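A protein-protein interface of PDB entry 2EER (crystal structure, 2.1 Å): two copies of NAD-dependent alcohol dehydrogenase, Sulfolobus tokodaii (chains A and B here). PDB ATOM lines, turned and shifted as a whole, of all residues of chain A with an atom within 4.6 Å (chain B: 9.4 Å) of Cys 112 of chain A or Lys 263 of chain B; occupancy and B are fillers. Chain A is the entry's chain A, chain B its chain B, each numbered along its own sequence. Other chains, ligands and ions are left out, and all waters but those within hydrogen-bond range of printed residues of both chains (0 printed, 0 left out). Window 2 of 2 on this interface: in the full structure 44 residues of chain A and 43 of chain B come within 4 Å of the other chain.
OH of Tyr 103 of chain A is in hydrogen-bond range of O of Lys 263 of chain B, at 2.8 Å. The side-chain carboxylate (OE2) of Glu 108 of chain A is in hydrogen-bond range of the side-chain amide nitrogen (NE2) of Gln 264 of chain B, 2.9 Å away. NE2 of His 110 of chain A sits at hydrogen-bond distance from OE2 of Glu 288 of chain B (3.4 Å). The backbone carbonyl oxygen (O) of Leu 111 of chain A lies within hydrogen-bond range of the side-chain amino group (NZ) of Lys 263 of chain B. The backbone carbonyl oxygen (O) of Cys 112 of chain A is in hydrogen-bond range of the side-chain amino group (NZ) of Lys 263 of chain B, 3.4 Å away. OD1 of Asp 113 of chain A lies within salt-bridge range of NZ of Lys 263 of chain B.
The backbone NH of Tyr 103 of chain A sits close to the side-chain sulfur of Cys 101 of chain A (3.5 Å). SG of Cys 101 of chain A lies close to N of Asp 113 of chain A, 3.5 Å away. SG of Cys 112 of chain A sits close to N of Ser 114 of chain A. N of Ala 262 of chain B is in hydrogen-bond range of O of Ala 241 of chain B (2.7 Å). The backbone NH (N) of Gln 264 of chain B sits at hydrogen-bond distance from the backbone carbonyl oxygen (O) of Asn 287 of chain B. OE1 of Glu 288 of chain B sits at hydrogen-bond distance from NE2 of Gln 264 of chain B (3.4 Å).
Among the printed residues, pairs that only touch across the chains: Tyr 103 of chain A with Lys 239 of chain B, Tyr 103 of chain A with Ala 262 of chain B, Tyr 103 of chain A with Gln 264 of chain B, Leu 111 of chain A with Gln 264 of chain B and Leu 111 of chain A with Glu 288 of chain B.
Cys 112 of chain A touches one residue of chain B. Lys 263 of chain B touches just these residues of chain A: Tyr 103, Leu 111, Cys 112 and Asp 113. Leu 111 of chain A touches three residues of chain B. Asp 113 of chain A touches just one residue of chain B: Lys 263 (2.9 Å). No residue of chain B comes within 4 Å of Ser 114 of chain A. Printed residues of chain A within 4 Å of Ala 262 of chain B: Tyr 103. Printed residues of chain B within 4 Å of Tyr 103 of chain A: Lys 239, Ala 262, Lys 263 and Gln 264. Of the printed residues of chain A, Gln 264 of chain B touches Tyr 103, Glu 108 and Leu 111. Val 289 of chain B touches none of the printed residues of chain A. The nearest printed residue of chain A that does not touch Lys 263 of chain B is Ser 114 of chain A (5.8 Å). The nearest printed residue of chain A that does not touch Glu 288 of chain B is Glu 108 of chain A (5.0 Å).
Of the 13 printed residues of chain A, 6 touch a printed residue of chain B. Hydrophobic or aromatic side chains of chain B within 4 Å of the printed part of chain A: Ala 262.
No position is printed for both chains.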
ATOM      1  N   GLY A  97     -16.132 -15.042  18.725  1.00  0.00           N
ATOM      2  CA  GLY A  97     -15.193 -13.956  18.964  1.00  0.00           C
ATOM      3  C   GLY A  97     -13.756 -14.369  18.694  1.00  0.00           C
ATOM      4  O   GLY A  97     -13.478 -15.551  18.497  1.00  0.00           O
ATOM      5  N   GLU A  98     -12.837 -13.405  18.701  1.00  0.00           N
ATOM      6  CA  GLU A  98     -11.427 -13.688  18.422  1.00  0.00           C
ATOM      7  C   GLU A  98     -10.561 -14.046  19.638  1.00  0.00           C
ATOM      8  O   GLU A  98      -9.438 -14.531  19.479  1.00  0.00           O
ATOM      9  CB  GLU A  98     -10.812 -12.516  17.647  1.00  0.00           C
ATOM     10  CG  GLU A  98     -11.112 -11.162  18.253  1.00  0.00           C
ATOM     11  CD  GLU A  98     -10.402 -10.957  19.570  1.00  0.00           C
ATOM     12  OE1 GLU A  98      -9.259 -11.441  19.706  1.00  0.00           O
ATOM     13  OE2 GLU A  98     -10.982 -10.307  20.463  1.00  0.00           O
ATOM     14  N   CYS A 101      -9.812  -9.494  22.828  1.00  0.00           N
ATOM     15  CA  CYS A 101     -10.435  -8.281  23.359  1.00  0.00           C
ATOM     16  C   CYS A 101     -11.049  -8.464  24.748  1.00  0.00           C
ATOM     17  O   CYS A 101     -11.268  -9.591  25.205  1.00  0.00           O
ATOM     18  CB  CYS A 101     -11.513  -7.768  22.403  1.00  0.00           C
ATOM     19  SG  CYS A 101     -13.094  -8.613  22.583  1.00  0.00           S
ATOM     20  N   TYR A 103     -14.020  -8.218  25.976  1.00  0.00           N
ATOM     21  CA  TYR A 103     -15.213  -9.054  26.045  1.00  0.00           C
ATOM     22  C   TYR A 103     -14.960 -10.555  25.918  1.00  0.00           C
ATOM     23  O   TYR A 103     -15.601 -11.353  26.606  1.00  0.00           O
ATOM     24  CB  TYR A 103     -16.227  -8.550  25.015  1.00  0.00           C
ATOM     25  CG  TYR A 103     -16.702  -7.155  25.369  1.00  0.00           C
ATOM     26  CD1 TYR A 103     -17.604  -6.953  26.413  1.00  0.00           C
ATOM     27  CD2 TYR A 103     -16.176  -6.032  24.725  1.00  0.00           C
ATOM     28  CE1 TYR A 103     -17.969  -5.670  26.815  1.00  0.00           C
ATOM     29  CE2 TYR A 103     -16.531  -4.742  25.120  1.00  0.00           C
ATOM     30  CZ  TYR A 103     -17.425  -4.570  26.167  1.00  0.00           C
ATOM     31  OH  TYR A 103     -17.764  -3.308  26.576  1.00  0.00           O
ATOM     32  N   CYS A 104     -14.030 -10.949  25.056  1.00  0.00           N
ATOM     33  CA  CYS A 104     -13.721 -12.367  24.931  1.00  0.00           C
ATOM     34  C   CYS A 104     -13.053 -12.843  26.228  1.00  0.00           C
ATOM     35  O   CYS A 104     -13.341 -13.936  26.728  1.00  0.00           O
ATOM     36  CB  CYS A 104     -12.800 -12.611  23.734  1.00  0.00           C
ATOM     37  SG  CYS A 104     -13.650 -12.544  22.147  1.00  0.00           S
ATOM     38  N   GLU A 108     -17.640 -13.151  27.364  1.00  0.00           N
ATOM     39  CA  GLU A 108     -18.796 -12.575  26.679  1.00  0.00           C
ATOM     40  C   GLU A 108     -18.402 -12.441  25.205  1.00  0.00           C
ATOM     41  O   GLU A 108     -18.448 -11.351  24.632  1.00  0.00           O
ATOM     42  CB  GLU A 108     -19.130 -11.198  27.274  1.00  0.00           C
ATOM     43  CG  GLU A 108     -19.518 -11.239  28.749  1.00  0.00           C
ATOM     44  CD  GLU A 108     -20.868 -11.897  28.989  1.00  0.00           C
ATOM     45  OE1 GLU A 108     -21.182 -12.897  28.312  1.00  0.00           O
ATOM     46  OE2 GLU A 108     -21.617 -11.421  29.864  1.00  0.00           O
ATOM     47  N   GLU A 109     -18.014 -13.569  24.614  1.00  0.00           N
ATOM     48  CA  GLU A 109     -17.560 -13.640  23.224  1.00  0.00           C
ATOM     49  C   GLU A 109     -18.470 -13.023  22.173  1.00  0.00           C
ATOM     50  O   GLU A 109     -17.988 -12.474  21.181  1.00  0.00           O
ATOM     51  CB  GLU A 109     -17.290 -15.097  22.834  1.00  0.00           C
ATOM     52  CG  GLU A 109     -16.095 -15.707  23.541  1.00  0.00           C
ATOM     53  CD  GLU A 109     -15.885 -17.160  23.178  1.00  0.00           C
ATOM     54  OE1 GLU A 109     -15.769 -17.457  21.968  1.00  0.00           O
ATOM     55  OE2 GLU A 109     -15.829 -18.002  24.099  1.00  0.00           O
ATOM     56  N   HIS A 110     -19.777 -13.124  22.378  1.00  0.00           N
ATOM     57  CA  HIS A 110     -20.721 -12.576  21.417  1.00  0.00           C
ATOM     58  C   HIS A 110     -20.602 -11.056  21.308  1.00  0.00           C
ATOM     59  O   HIS A 110     -21.032 -10.470  20.318  1.00  0.00           O
ATOM     60  CB  HIS A 110     -22.152 -12.981  21.790  1.00  0.00           C
ATOM     61  CG  HIS A 110     -22.608 -12.461  23.117  1.00  0.00           C
ATOM     62  ND1 HIS A 110     -21.948 -12.741  24.294  1.00  0.00           N
ATOM     63  CD2 HIS A 110     -23.679 -11.705  23.456  1.00  0.00           C
ATOM     64  CE1 HIS A 110     -22.594 -12.181  25.302  1.00  0.00           C
ATOM     65  NE2 HIS A 110     -23.649 -11.546  24.821  1.00  0.00           N
ATOM     66  N   LEU A 111     -20.005 -10.425  22.316  1.00  0.00           N
ATOM     67  CA  LEU A 111     -19.831  -8.971  22.316  1.00  0.00           C
ATOM     68  C   LEU A 111     -18.414  -8.576  21.896  1.00  0.00           C
ATOM     69  O   LEU A 111     -17.965  -7.456  22.142  1.00  0.00           O
ATOM     70  CB  LEU A 111     -20.149  -8.401  23.703  1.00  0.00           C
ATOM     71  CG  LEU A 111     -21.616  -8.549  24.129  1.00  0.00           C
ATOM     72  CD1 LEU A 111     -21.791  -8.090  25.562  1.00  0.00           C
ATOM     73  CD2 LEU A 111     -22.500  -7.729  23.206  1.00  0.00           C
ATOM     74  N   CYS A 112     -17.719  -9.512  21.259  1.00  0.00           N
ATOM     75  CA  CYS A 112     -16.361  -9.289  20.785  1.00  0.00           C
ATOM     76  C   CYS A 112     -16.277  -7.995  19.977  1.00  0.00           C
ATOM     77  O   CYS A 112     -17.229  -7.628  19.286  1.00  0.00           O
ATOM     78  CB  CYS A 112     -15.926 -10.473  19.917  1.00  0.00           C
ATOM     79  SG  CYS A 112     -14.306 -10.300  19.136  1.00  0.00           S
ATOM     80  N   ASP A 113     -15.142  -7.305  20.072  1.00  0.00           N
ATOM     81  CA  ASP A 113     -14.946  -6.057  19.331  1.00  0.00           C
ATOM     82  C   ASP A 113     -14.755  -6.342  17.841  1.00  0.00           C
ATOM     83  O   ASP A 113     -15.026  -5.493  16.992  1.00  0.00           O
ATOM     84  CB  ASP A 113     -13.726  -5.289  19.860  1.00  0.00           C
ATOM     85  CG  ASP A 113     -13.931  -4.764  21.271  1.00  0.00           C
ATOM     86  OD1 ASP A 113     -15.075  -4.397  21.610  1.00  0.00           O
ATOM     87  OD2 ASP A 113     -12.945  -4.701  22.035  1.00  0.00           O
ATOM     88  N   SER A 114     -14.279  -7.541  17.529  1.00  0.00           N
ATOM     89  CA  SER A 114     -14.066  -7.947  16.146  1.00  0.00           C
ATOM     90  C   SER A 114     -14.864  -9.227  15.941  1.00  0.00           C
ATOM     91  O   SER A 114     -14.300 -10.283  15.670  1.00  0.00           O
ATOM     92  CB  SER A 114     -12.579  -8.198  15.910  1.00  0.00           C
ATOM     93  OG  SER A 114     -11.826  -7.036  16.223  1.00  0.00           O
ATOM     94  N   PRO A 115     -16.201  -9.137  16.059  1.00  0.00           N
ATOM     95  CA  PRO A 115     -17.139 -10.253  15.911  1.00  0.00           C
ATOM     96  C   PRO A 115     -17.101 -11.045  14.613  1.00  0.00           C
ATOM     97  O   PRO A 115     -16.884 -10.500  13.527  1.00  0.00           O
ATOM     98  CB  PRO A 115     -18.494  -9.590  16.133  1.00  0.00           C
ATOM     99  CG  PRO A 115     -18.284  -8.229  15.558  1.00  0.00           C
ATOM    100  CD  PRO A 115     -16.937  -7.862  16.138  1.00  0.00           C
ATOM    101  N   LYS B 172     -12.815  -1.947  34.875  1.00  0.00           N
ATOM    102  CA  LYS B 172     -13.901  -1.046  34.499  1.00  0.00           C
ATOM    103  C   LYS B 172     -13.721   0.421  34.899  1.00  0.00           C
ATOM    104  O   LYS B 172     -12.969   0.749  35.821  1.00  0.00           O
ATOM    105  CB  LYS B 172     -15.215  -1.558  35.084  1.00  0.00           C
ATOM    106  CG  LYS B 172     -15.665  -2.897  34.532  1.00  0.00           C
ATOM    107  CD  LYS B 172     -17.021  -3.269  35.103  1.00  0.00           C
ATOM    108  CE  LYS B 172     -17.549  -4.550  34.492  1.00  0.00           C
ATOM    109  NZ  LYS B 172     -18.934  -4.807  34.958  1.00  0.00           N
ATOM    110  N   GLY B 238     -11.669   5.016  23.887  1.00  0.00           N
ATOM    111  CA  GLY B 238     -12.692   4.667  22.917  1.00  0.00           C
ATOM    112  C   GLY B 238     -13.682   3.589  23.327  1.00  0.00           C
ATOM    113  O   GLY B 238     -14.676   3.352  22.630  1.00  0.00           O
ATOM    114  N   LYS B 239     -13.424   2.928  24.450  1.00  0.00           N
ATOM    115  CA  LYS B 239     -14.320   1.872  24.907  1.00  0.00           C
ATOM    116  C   LYS B 239     -15.645   2.415  25.422  1.00  0.00           C
ATOM    117  O   LYS B 239     -16.707   1.854  25.149  1.00  0.00           O
ATOM    118  CB  LYS B 239     -13.670   1.044  26.016  1.00  0.00           C
ATOM    119  CG  LYS B 239     -14.525  -0.147  26.423  1.00  0.00           C
ATOM    120  CD  LYS B 239     -14.040  -0.804  27.700  1.00  0.00           C
ATOM    121  CE  LYS B 239     -14.896  -2.023  28.035  1.00  0.00           C
ATOM    122  NZ  LYS B 239     -14.568  -2.604  29.367  1.00  0.00           N
ATOM    123  N   GLY B 240     -15.579   3.511  26.166  1.00  0.00           N
ATOM    124  CA  GLY B 240     -16.778   4.088  26.745  1.00  0.00           C
ATOM    125  C   GLY B 240     -16.805   3.702  28.214  1.00  0.00           C
ATOM    126  O   GLY B 240     -15.984   2.896  28.660  1.00  0.00           O
ATOM    127  N   ALA B 241     -17.746   4.258  28.968  1.00  0.00           N
ATOM    128  CA  ALA B 241     -17.844   3.968  30.403  1.00  0.00           C
ATOM    129  C   ALA B 241     -18.575   2.651  30.679  1.00  0.00           C
ATOM    130  O   ALA B 241     -19.619   2.352  30.108  1.00  0.00           O
ATOM    131  CB  ALA B 241     -18.595   5.112  31.084  1.00  0.00           C
ATOM    132  N   ASP B 242     -17.970   1.834  31.563  1.00  0.00           N
ATOM    133  CA  ASP B 242     -18.605   0.567  31.899  1.00  0.00           C
ATOM    134  C   ASP B 242     -19.803   0.791  32.834  1.00  0.00           C
ATOM    135  O   ASP B 242     -20.700  -0.029  32.962  1.00  0.00           O
ATOM    136  CB  ASP B 242     -17.576  -0.355  32.568  1.00  0.00           C
ATOM    137  CG  ASP B 242     -16.434  -0.653  31.601  1.00  0.00           C
ATOM    138  OD1 ASP B 242     -16.647  -1.431  30.670  1.00  0.00           O
ATOM    139  OD2 ASP B 242     -15.340  -0.133  31.799  1.00  0.00           O
ATOM    140  N   ALA B 243     -19.764   1.936  33.537  1.00  0.00           N
ATOM    141  CA  ALA B 243     -20.876   2.274  34.413  1.00  0.00           C
ATOM    142  C   ALA B 243     -20.953   3.779  34.626  1.00  0.00           C
ATOM    143  O   ALA B 243     -19.951   4.475  34.687  1.00  0.00           O
ATOM    144  CB  ALA B 243     -20.665   1.577  35.757  1.00  0.00           C
ATOM    145  N   PRO B 258     -26.058   8.665  28.413  1.00  0.00           N
ATOM    146  CA  PRO B 258     -26.457   7.307  28.029  1.00  0.00           C
ATOM    147  C   PRO B 258     -25.750   6.886  26.734  1.00  0.00           C
ATOM    148  O   PRO B 258     -25.699   5.705  26.396  1.00  0.00           O
ATOM    149  CB  PRO B 258     -27.967   7.432  27.851  1.00  0.00           C
ATOM    150  CG  PRO B 258     -28.334   8.451  28.887  1.00  0.00           C
ATOM    151  CD  PRO B 258     -27.233   9.489  28.750  1.00  0.00           C
ATOM    152  N   TYR B 259     -25.198   7.865  26.019  1.00  0.00           N
ATOM    153  CA  TYR B 259     -24.512   7.611  24.750  1.00  0.00           C
ATOM    154  C   TYR B 259     -23.005   7.358  24.836  1.00  0.00           C
ATOM    155  O   TYR B 259     -22.354   7.154  23.808  1.00  0.00           O
ATOM    156  CB  TYR B 259     -24.786   8.767  23.783  1.00  0.00           C
ATOM    157  CG  TYR B 259     -26.254   8.922  23.485  1.00  0.00           C
ATOM    158  CD1 TYR B 259     -26.901   8.052  22.607  1.00  0.00           C
ATOM    159  CD2 TYR B 259     -27.018   9.882  24.145  1.00  0.00           C
ATOM    160  CE1 TYR B 259     -28.279   8.132  22.398  1.00  0.00           C
ATOM    161  CE2 TYR B 259     -28.392   9.967  23.948  1.00  0.00           C
ATOM    162  CZ  TYR B 259     -29.018   9.088  23.075  1.00  0.00           C
ATOM    163  OH  TYR B 259     -30.380   9.148  22.906  1.00  0.00           O
ATOM    164  N   VAL B 260     -22.445   7.375  26.043  1.00  0.00           N
ATOM    165  CA  VAL B 260     -21.012   7.119  26.208  1.00  0.00           C
ATOM    166  C   VAL B 260     -20.792   5.822  26.975  1.00  0.00           C
ATOM    167  O   VAL B 260     -19.739   5.607  27.575  1.00  0.00           O
ATOM    168  CB  VAL B 260     -20.286   8.269  26.964  1.00  0.00           C
ATOM    169  CG1 VAL B 260     -20.512   9.583  26.244  1.00  0.00           C
ATOM    170  CG2 VAL B 260     -20.764   8.348  28.409  1.00  0.00           C
ATOM    171  N   LEU B 261     -21.800   4.958  26.955  1.00  0.00           N
ATOM    172  CA  LEU B 261     -21.719   3.675  27.643  1.00  0.00           C
ATOM    173  C   LEU B 261     -20.960   2.656  26.812  1.00  0.00           C
ATOM    174  O   LEU B 261     -21.082   2.627  25.590  1.00  0.00           O
ATOM    175  CB  LEU B 261     -23.123   3.126  27.906  1.00  0.00           C
ATOM    176  CG  LEU B 261     -23.934   3.785  29.016  1.00  0.00           C
ATOM    177  CD1 LEU B 261     -25.379   3.323  28.934  1.00  0.00           C
ATOM    178  CD2 LEU B 261     -23.318   3.420  30.364  1.00  0.00           C
ATOM    179  N   ALA B 262     -20.174   1.819  27.474  1.00  0.00           N
ATOM    180  CA  ALA B 262     -19.454   0.766  26.775  1.00  0.00           C
ATOM    181  C   ALA B 262     -20.471  -0.358  26.617  1.00  0.00           C
ATOM    182  O   ALA B 262     -21.556  -0.304  27.206  1.00  0.00           O
ATOM    183  CB  ALA B 262     -18.279   0.289  27.609  1.00  0.00           C
ATOM    184  N   LYS B 263     -20.141  -1.368  25.818  1.00  0.00           N
ATOM    185  CA  LYS B 263     -21.053  -2.489  25.702  1.00  0.00           C
ATOM    186  C   LYS B 263     -21.191  -3.121  27.076  1.00  0.00           C
ATOM    187  O   LYS B 263     -20.241  -3.178  27.847  1.00  0.00           O
ATOM    188  CB  LYS B 263     -20.479  -3.498  24.696  1.00  0.00           C
ATOM    189  CG  LYS B 263     -20.639  -3.089  23.214  1.00  0.00           C
ATOM    190  CD  LYS B 263     -19.979  -4.086  22.235  1.00  0.00           C
ATOM    191  CE  LYS B 263     -18.446  -4.010  22.277  1.00  0.00           C
ATOM    192  NZ  LYS B 263     -17.862  -4.944  21.321  1.00  0.00           N
ATOM    193  N   GLN B 264     -22.441  -3.514  27.405  1.00  0.00           N
ATOM    194  CA  GLN B 264     -22.752  -4.065  28.728  1.00  0.00           C
ATOM    195  C   GLN B 264     -22.764  -2.998  29.835  1.00  0.00           C
ATOM    196  O   GLN B 264     -22.930  -3.281  31.008  1.00  0.00           O
ATOM    197  CB  GLN B 264     -21.762  -5.193  29.083  1.00  0.00           C
ATOM    198  CG  GLN B 264     -22.030  -6.483  28.299  1.00  0.00           C
ATOM    199  CD  GLN B 264     -21.362  -7.660  28.982  1.00  0.00           C
ATOM    200  OE1 GLN B 264     -20.151  -7.712  29.188  1.00  0.00           O
ATOM    201  NE2 GLN B 264     -22.203  -8.657  29.297  1.00  0.00           N
ATOM    202  N   GLY B 265     -22.534  -1.735  29.411  1.00  0.00           N
ATOM    203  CA  GLY B 265     -22.480  -0.640  30.381  1.00  0.00           C
ATOM    204  C   GLY B 265     -23.796  -0.518  31.176  1.00  0.00           C
ATOM    205  O   GLY B 265     -24.884  -0.731  30.670  1.00  0.00           O
ATOM    206  N   LYS B 266     -23.655  -0.158  32.447  1.00  0.00           N
ATOM    207  CA  LYS B 266     -24.805   0.022  33.320  1.00  0.00           C
ATOM    208  C   LYS B 266     -24.999   1.494  33.682  1.00  0.00           C
ATOM    209  O   LYS B 266     -24.102   2.138  34.227  1.00  0.00           O
ATOM    210  CB  LYS B 266     -24.632  -0.797  34.605  1.00  0.00           C
ATOM    211  CG  LYS B 266     -24.545  -2.305  34.388  1.00  0.00           C
ATOM    212  CD  LYS B 266     -24.480  -3.034  35.721  1.00  0.00           C
ATOM    213  CE  LYS B 266     -24.441  -4.540  35.539  1.00  0.00           C
ATOM    214  NZ  LYS B 266     -23.226  -4.941  34.783  1.00  0.00           N
ATOM    215  N   TYR B 279     -34.547   6.762  24.570  1.00  0.00           N
ATOM    216  CA  TYR B 279     -33.379   6.071  24.044  1.00  0.00           C
ATOM    217  C   TYR B 279     -33.813   5.036  23.006  1.00  0.00           C
ATOM    218  O   TYR B 279     -34.761   4.285  23.240  1.00  0.00           O
ATOM    219  CB  TYR B 279     -32.656   5.384  25.203  1.00  0.00           C
ATOM    220  CG  TYR B 279     -31.204   5.057  24.945  1.00  0.00           C
ATOM    221  CD1 TYR B 279     -30.231   6.055  24.972  1.00  0.00           C
ATOM    222  CD2 TYR B 279     -30.799   3.747  24.703  1.00  0.00           C
ATOM    223  CE1 TYR B 279     -28.884   5.754  24.769  1.00  0.00           C
ATOM    224  CE2 TYR B 279     -29.460   3.433  24.497  1.00  0.00           C
ATOM    225  CZ  TYR B 279     -28.508   4.440  24.533  1.00  0.00           C
ATOM    226  OH  TYR B 279     -27.181   4.133  24.335  1.00  0.00           O
ATOM    227  N   LEU B 283     -30.462   0.224  20.383  1.00  0.00           N
ATOM    228  CA  LEU B 283     -29.189   0.581  21.001  1.00  0.00           C
ATOM    229  C   LEU B 283     -29.040  -0.174  22.308  1.00  0.00           C
ATOM    230  O   LEU B 283     -27.945  -0.589  22.674  1.00  0.00           O
ATOM    231  CB  LEU B 283     -29.113   2.083  21.280  1.00  0.00           C
ATOM    232  CG  LEU B 283     -28.862   2.995  20.079  1.00  0.00           C
ATOM    233  CD1 LEU B 283     -28.845   4.454  20.543  1.00  0.00           C
ATOM    234  CD2 LEU B 283     -27.542   2.626  19.422  1.00  0.00           C
ATOM    235  N   ILE B 284     -30.153  -0.349  23.013  1.00  0.00           N
ATOM    236  CA  ILE B 284     -30.137  -1.067  24.279  1.00  0.00           C
ATOM    237  C   ILE B 284     -29.845  -2.547  24.043  1.00  0.00           C
ATOM    238  O   ILE B 284     -28.976  -3.133  24.680  1.00  0.00           O
ATOM    239  CB  ILE B 284     -31.492  -0.931  25.007  1.00  0.00           C
ATOM    240  CG1 ILE B 284     -31.731   0.536  25.382  1.00  0.00           C
ATOM    241  CG2 ILE B 284     -31.510  -1.824  26.250  1.00  0.00           C
ATOM    242  CD1 ILE B 284     -33.073   0.805  26.044  1.00  0.00           C
ATOM    243  N   THR B 285     -30.564  -3.139  23.101  1.00  0.00           N
ATOM    244  CA  THR B 285     -30.409  -4.553  22.778  1.00  0.00           C
ATOM    245  C   THR B 285     -29.039  -4.934  22.210  1.00  0.00           C
ATOM    246  O   THR B 285     -28.350  -5.812  22.741  1.00  0.00           O
ATOM    247  CB  THR B 285     -31.496  -4.978  21.772  1.00  0.00           C
ATOM    248  OG1 THR B 285     -32.782  -4.622  22.298  1.00  0.00           O
ATOM    249  CG2 THR B 285     -31.448  -6.484  21.518  1.00  0.00           C
ATOM    250  N   LEU B 286     -28.645  -4.269  21.131  1.00  0.00           N
ATOM    251  CA  LEU B 286     -27.382  -4.569  20.467  1.00  0.00           C
ATOM    252  C   LEU B 286     -26.122  -4.297  21.293  1.00  0.00           C
ATOM    253  O   LEU B 286     -25.072  -4.882  21.029  1.00  0.00           O
ATOM    254  CB  LEU B 286     -27.312  -3.814  19.137  1.00  0.00           C
ATOM    255  CG  LEU B 286     -28.467  -4.097  18.165  1.00  0.00           C
ATOM    256  CD1 LEU B 286     -28.231  -3.332  16.869  1.00  0.00           C
ATOM    257  CD2 LEU B 286     -28.578  -5.589  17.883  1.00  0.00           C
ATOM    258  N   ASN B 287     -26.219  -3.422  22.289  1.00  0.00           N
ATOM    259  CA  ASN B 287     -25.063  -3.122  23.129  1.00  0.00           C
ATOM    260  C   ASN B 287     -25.205  -3.690  24.537  1.00  0.00           C
ATOM    261  O   ASN B 287     -24.327  -3.494  25.374  1.00  0.00           O
ATOM    262  CB  ASN B 287     -24.845  -1.609  23.208  1.00  0.00           C
ATOM    263  CG  ASN B 287     -24.521  -0.994  21.855  1.00  0.00           C
ATOM    264  OD1 ASN B 287     -23.577  -1.412  21.184  1.00  0.00           O
ATOM    265  ND2 ASN B 287     -25.304  -0.001  21.447  1.00  0.00           N
ATOM    266  N   GLU B 288     -26.303  -4.404  24.787  1.00  0.00           N
ATOM    267  CA  GLU B 288     -26.582  -4.987  26.100  1.00  0.00           C
ATOM    268  C   GLU B 288     -26.422  -3.969  27.220  1.00  0.00           C
ATOM    269  O   GLU B 288     -25.965  -4.290  28.319  1.00  0.00           O
ATOM    270  CB  GLU B 288     -25.682  -6.195  26.387  1.00  0.00           C
ATOM    271  CG  GLU B 288     -26.014  -7.433  25.566  1.00  0.00           C
ATOM    272  CD  GLU B 288     -25.779  -8.735  26.331  1.00  0.00           C
ATOM    273  OE1 GLU B 288     -25.008  -8.736  27.318  1.00  0.00           O
ATOM    274  OE2 GLU B 288     -26.359  -9.766  25.933  1.00  0.00           O
ATOM    275  N   VAL B 289     -26.795  -2.734  26.928  1.00  0.00           N
ATOM    276  CA  VAL B 289     -26.714  -1.666  27.910  1.00  0.00           C
ATOM    277  C   VAL B 289     -27.826  -1.861  28.934  1.00  0.00           C
ATOM    278  O   VAL B 289     -28.815  -2.542  28.656  1.00  0.00           O
ATOM    279  CB  VAL B 289     -26.843  -0.301  27.195  1.00  0.00           C
ATOM    280  CG1 VAL B 289     -27.549   0.719  28.081  1.00  0.00           C
ATOM    281  CG2 VAL B 289     -25.451   0.181  26.794  1.00  0.00           C
ATOM    282  N   GLN B 290     -27.662  -1.285  30.122  1.00  0.00           N
ATOM    283  CA  GLN B 290     -28.682  -1.402  31.153  1.00  0.00           C
ATOM    284  C   GLN B 290     -28.998  -0.065  31.814  1.00  0.00           C
ATOM    285  O   GLN B 290     -28.099   0.719  32.111  1.00  0.00           O
ATOM    286  CB  GLN B 290     -28.242  -2.390  32.241  1.00  0.00           C
ATOM    287  CG  GLN B 290     -28.051  -3.814  31.754  1.00  0.00           C
ATOM    288  CD  GLN B 290     -27.712  -4.776  32.874  1.00  0.00           C
ATOM    289  OE1 GLN B 290     -28.003  -4.515  34.039  1.00  0.00           O
ATOM    290  NE2 GLN B 290     -27.110  -5.905  32.522  1.00  0.00           N
